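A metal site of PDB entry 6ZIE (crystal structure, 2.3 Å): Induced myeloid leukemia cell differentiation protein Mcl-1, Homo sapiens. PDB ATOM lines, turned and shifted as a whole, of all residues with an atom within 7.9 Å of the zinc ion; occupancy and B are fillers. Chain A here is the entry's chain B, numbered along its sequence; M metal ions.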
ATOM      1  N   LEU A  67     -13.152 -21.456  11.320  1.00  0.00           N
ATOM      2  CA  LEU A  67     -12.155 -20.504  11.802  1.00  0.00           C
ATOM      3  C   LEU A  67     -12.725 -19.102  11.932  1.00  0.00           C
ATOM      4  O   LEU A  67     -12.484 -18.430  12.938  1.00  0.00           O
ATOM      5  CB  LEU A  67     -10.940 -20.520  10.866  1.00  0.00           C
ATOM      6  CG  LEU A  67      -9.829 -19.518  11.166  1.00  0.00           C
ATOM      7  CD1 LEU A  67      -9.242 -19.738  12.562  1.00  0.00           C
ATOM      8  CD2 LEU A  67      -8.735 -19.609  10.134  1.00  0.00           C
ATOM      9  N   ARG A  68     -13.561 -18.681  10.976  1.00  0.00           N
ATOM     10  CA  ARG A  68     -14.198 -17.368  11.023  1.00  0.00           C
ATOM     11  C   ARG A  68     -15.150 -17.201  12.211  1.00  0.00           C
ATOM     12  O   ARG A  68     -15.315 -16.093  12.712  1.00  0.00           O
ATOM     13  CB  ARG A  68     -14.898 -17.052   9.696  1.00  0.00           C
ATOM     14  CG  ARG A  68     -13.940 -16.848   8.522  1.00  0.00           C
ATOM     15  CD  ARG A  68     -12.993 -15.670   8.731  1.00  0.00           C
ATOM     16  NE  ARG A  68     -13.717 -14.428   8.960  1.00  0.00           N
ATOM     17  CZ  ARG A  68     -13.155 -13.263   9.277  1.00  0.00           C
ATOM     18  NH1 ARG A  68     -11.828 -13.186   9.413  1.00  0.00           N
ATOM     19  NH2 ARG A  68     -13.887 -12.179   9.475  1.00  0.00           N
ATOM     20  N   LEU A  70     -14.522 -18.500  15.138  1.00  0.00           N
ATOM     21  CA  LEU A  70     -13.658 -18.412  16.314  1.00  0.00           C
ATOM     22  C   LEU A  70     -13.048 -17.008  16.415  1.00  0.00           C
ATOM     23  O   LEU A  70     -12.891 -16.484  17.507  1.00  0.00           O
ATOM     24  CB  LEU A  70     -12.535 -19.464  16.261  1.00  0.00           C
ATOM     25  CG  LEU A  70     -12.950 -20.926  16.019  1.00  0.00           C
ATOM     26  CD1 LEU A  70     -11.752 -21.845  16.117  1.00  0.00           C
ATOM     27  CD2 LEU A  70     -14.016 -21.386  17.011  1.00  0.00           C
ATOM     28  N   ASP A  71     -12.690 -16.411  15.261  1.00  0.00           N
ATOM     29  CA  ASP A  71     -12.105 -15.077  15.211  1.00  0.00           C
ATOM     30  C   ASP A  71     -13.100 -14.028  15.656  1.00  0.00           C
ATOM     31  O   ASP A  71     -12.687 -13.060  16.308  1.00  0.00           O
ATOM     32  CB  ASP A  71     -11.662 -14.738  13.788  1.00  0.00           C
ATOM     33  CG  ASP A  71     -10.361 -15.361  13.358  1.00  0.00           C
ATOM     34  OD1 ASP A  71      -9.578 -15.760  14.243  1.00  0.00           O
ATOM     35  OD2 ASP A  71     -10.112 -15.430  12.136  1.00  0.00           O
ATOM     36  N   ILE A  72     -14.405 -14.188  15.304  1.00  0.00           N
ATOM     37  CA  ILE A  72     -15.487 -13.261  15.642  1.00  0.00           C
ATOM     38  C   ILE A  72     -15.449 -12.839  17.128  1.00  0.00           C
ATOM     39  O   ILE A  72     -15.782 -11.695  17.450  1.00  0.00           O
ATOM     40  CB  ILE A  72     -16.872 -13.789  15.200  1.00  0.00           C
ATOM     41  CG1 ILE A  72     -17.875 -12.634  14.991  1.00  0.00           C
ATOM     42  CG2 ILE A  72     -17.417 -14.839  16.170  1.00  0.00           C
ATOM     43  CD1 ILE A  72     -19.196 -13.032  14.422  1.00  0.00           C
ATOM     44  N   LYS A  73     -14.975 -13.722  18.019  1.00  0.00           N
ATOM     45  CA  LYS A  73     -14.784 -13.404  19.423  1.00  0.00           C
ATOM     46  C   LYS A  73     -13.290 -13.177  19.568  1.00  0.00           C
ATOM     47  O   LYS A  73     -12.520 -14.122  19.391  1.00  0.00           O
ATOM     48  CB  LYS A  73     -15.331 -14.504  20.354  1.00  0.00           C
ATOM     49  CG  LYS A  73     -14.945 -15.950  19.995  1.00  0.00           C
ATOM     50  CD  LYS A  73     -15.743 -16.966  20.797  1.00  0.00           C
ATOM     51  CE  LYS A  73     -17.149 -17.082  20.266  1.00  0.00           C
ATOM     52  NZ  LYS A  73     -18.047 -17.741  21.245  1.00  0.00           N
ATOM     53  N   GLU A  75     -10.053 -13.294  20.615  1.00  0.00           N
ATOM     54  CA  GLU A  75      -9.404 -14.157  21.603  1.00  0.00           C
ATOM     55  C   GLU A  75      -8.290 -14.965  20.926  1.00  0.00           C
ATOM     56  O   GLU A  75      -8.243 -15.069  19.701  1.00  0.00           O
ATOM     57  CB  GLU A  75     -10.490 -15.128  22.130  1.00  0.00           C
ATOM     58  CG  GLU A  75     -10.097 -15.973  23.329  1.00  0.00           C
ATOM     59  CD  GLU A  75     -11.112 -17.025  23.732  1.00  0.00           C
ATOM     60  OE1 GLU A  75     -12.136 -17.184  23.030  1.00  0.00           O
ATOM     61  OE2 GLU A  75     -10.868 -17.712  24.754  1.00  0.00           O
ATOM     62  N   ASP A  76      -7.414 -15.594  21.735  1.00  0.00           N
ATOM     63  CA  ASP A  76      -6.356 -16.473  21.235  1.00  0.00           C
ATOM     64  C   ASP A  76      -7.069 -17.681  20.646  1.00  0.00           C
ATOM     65  O   ASP A  76      -7.786 -18.380  21.355  1.00  0.00           O
ATOM     66  CB  ASP A  76      -5.418 -16.860  22.392  1.00  0.00           C
ATOM     67  CG  ASP A  76      -4.162 -17.617  21.995  1.00  0.00           C
ATOM     68  OD1 ASP A  76      -4.176 -18.291  20.943  1.00  0.00           O
ATOM     69  OD2 ASP A  76      -3.177 -17.546  22.752  1.00  0.00           O
ATOM     70  N   ASP A  77      -6.968 -17.830  19.317  1.00  0.00           N
ATOM     71  CA  ASP A  77      -7.615 -18.867  18.528  1.00  0.00           C
ATOM     72  C   ASP A  77      -7.404 -20.283  19.050  1.00  0.00           C
ATOM     73  O   ASP A  77      -8.279 -21.133  18.887  1.00  0.00           O
ATOM     74  CB  ASP A  77      -7.186 -18.766  17.064  1.00  0.00           C
ATOM     75  CG  ASP A  77      -7.613 -17.490  16.360  1.00  0.00           C
ATOM     76  OD1 ASP A  77      -8.134 -16.572  17.042  1.00  0.00           O
ATOM     77  OD2 ASP A  77      -7.442 -17.409  15.133  1.00  0.00           O
ATOM     78  N   VAL A  78      -6.257 -20.545  19.686  1.00  0.00           N
ATOM     79  CA  VAL A  78      -5.909 -21.848  20.236  1.00  0.00           C
ATOM     80  C   VAL A  78      -6.772 -22.179  21.449  1.00  0.00           C
ATOM     81  O   VAL A  78      -7.226 -23.317  21.601  1.00  0.00           O
ATOM     82  CB  VAL A  78      -4.412 -21.863  20.604  1.00  0.00           C
ATOM     83  CG1 VAL A  78      -4.022 -23.201  21.203  1.00  0.00           C
ATOM     84  CG2 VAL A  78      -3.568 -21.537  19.376  1.00  0.00           C
ATOM     85  N   VAL A 109      -5.309 -24.153  11.175  1.00  0.00           N
ATOM     86  CA  VAL A 109      -5.275 -23.072  12.149  1.00  0.00           C
ATOM     87  C   VAL A 109      -3.843 -22.554  12.334  1.00  0.00           C
ATOM     88  O   VAL A 109      -3.640 -21.347  12.393  1.00  0.00           O
ATOM     89  CB  VAL A 109      -5.942 -23.508  13.492  1.00  0.00           C
ATOM     90  CG1 VAL A 109      -5.643 -22.519  14.621  1.00  0.00           C
ATOM     91  CG2 VAL A 109      -7.436 -23.699  13.334  1.00  0.00           C
ATOM     92  N   HIS A 112      -3.005 -20.037   9.725  1.00  0.00           N
ATOM     93  CA  HIS A 112      -3.653 -18.766  10.063  1.00  0.00           C
ATOM     94  C   HIS A 112      -2.853 -18.046  11.146  1.00  0.00           C
ATOM     95  O   HIS A 112      -2.656 -16.840  11.064  1.00  0.00           O
ATOM     96  CB  HIS A 112      -5.111 -19.025  10.494  1.00  0.00           C
ATOM     97  CG  HIS A 112      -5.769 -17.863  11.173  1.00  0.00           C
ATOM     98  ND1 HIS A 112      -6.157 -16.742  10.460  1.00  0.00           N
ATOM     99  CD2 HIS A 112      -6.081 -17.682  12.477  1.00  0.00           C
ATOM    100  CE1 HIS A 112      -6.694 -15.924  11.347  1.00  0.00           C
ATOM    101  NE2 HIS A 112      -6.676 -16.449  12.582  1.00  0.00           N
ATOM    102  N   LEU A 113      -2.351 -18.804  12.142  1.00  0.00           N
ATOM    103  CA  LEU A 113      -1.501 -18.269  13.211  1.00  0.00           C
ATOM    104  C   LEU A 113      -0.203 -17.709  12.616  1.00  0.00           C
ATOM    105  O   LEU A 113       0.283 -16.697  13.074  1.00  0.00           O
ATOM    106  CB  LEU A 113      -1.184 -19.348  14.251  1.00  0.00           C
ATOM    107  CG  LEU A 113      -2.357 -19.804  15.127  1.00  0.00           C
ATOM    108  CD1 LEU A 113      -1.954 -20.983  16.005  1.00  0.00           C
ATOM    109  CD2 LEU A 113      -2.887 -18.663  15.977  1.00  0.00           C
ATOM    110  N   ILE A 116      -1.107 -14.228  10.805  1.00  0.00           N
ATOM    111  CA  ILE A 116      -1.312 -13.105  11.726  1.00  0.00           C
ATOM    112  C   ILE A 116      -0.142 -12.862  12.703  1.00  0.00           C
ATOM    113  O   ILE A 116      -0.309 -12.117  13.666  1.00  0.00           O
ATOM    114  CB  ILE A 116      -2.648 -13.286  12.492  1.00  0.00           C
ATOM    115  CG1 ILE A 116      -2.574 -14.422  13.534  1.00  0.00           C
ATOM    116  CG2 ILE A 116      -3.814 -13.506  11.507  1.00  0.00           C
ATOM    117  CD1 ILE A 116      -3.805 -14.510  14.436  1.00  0.00           C
ATOM    118  N   GLN A 118       1.420 -15.009  14.924  1.00  0.00           N
ATOM    119  CA  GLN A 118       1.162 -15.608  16.223  1.00  0.00           C
ATOM    120  C   GLN A 118       1.671 -17.063  16.243  1.00  0.00           C
ATOM    121  O   GLN A 118       1.008 -17.937  16.797  1.00  0.00           O
ATOM    122  CB  GLN A 118      -0.346 -15.555  16.551  1.00  0.00           C
ATOM    123  CG  GLN A 118      -0.653 -15.560  18.034  1.00  0.00           C
ATOM    124  CD  GLN A 118      -2.139 -15.645  18.261  1.00  0.00           C
ATOM    125  OE1 GLN A 118      -2.923 -14.952  17.620  1.00  0.00           O
ATOM    126  NE2 GLN A 118      -2.545 -16.500  19.197  1.00  0.00           N
HETATM  127 ZN    ZN M   1      -7.556 -15.764  14.207  1.00  0.00          ZN
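OD2 of Asp 77 binds the zinc ion, 1.9 Å away. A ring nitrogen (NE2) of His 112 is bound to the zinc ion (2.0 Å). The zinc ion is bound by OD1 of Asp 71, 2.0 Å away. The zinc ion has three donor atoms within binding distance.
NH1 of Arg 68 is in salt-bridge range of OD2 of Asp 71, at 3.9 Å.
Merely in contact with the zinc ion: Ile 116 (3.96 Å).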
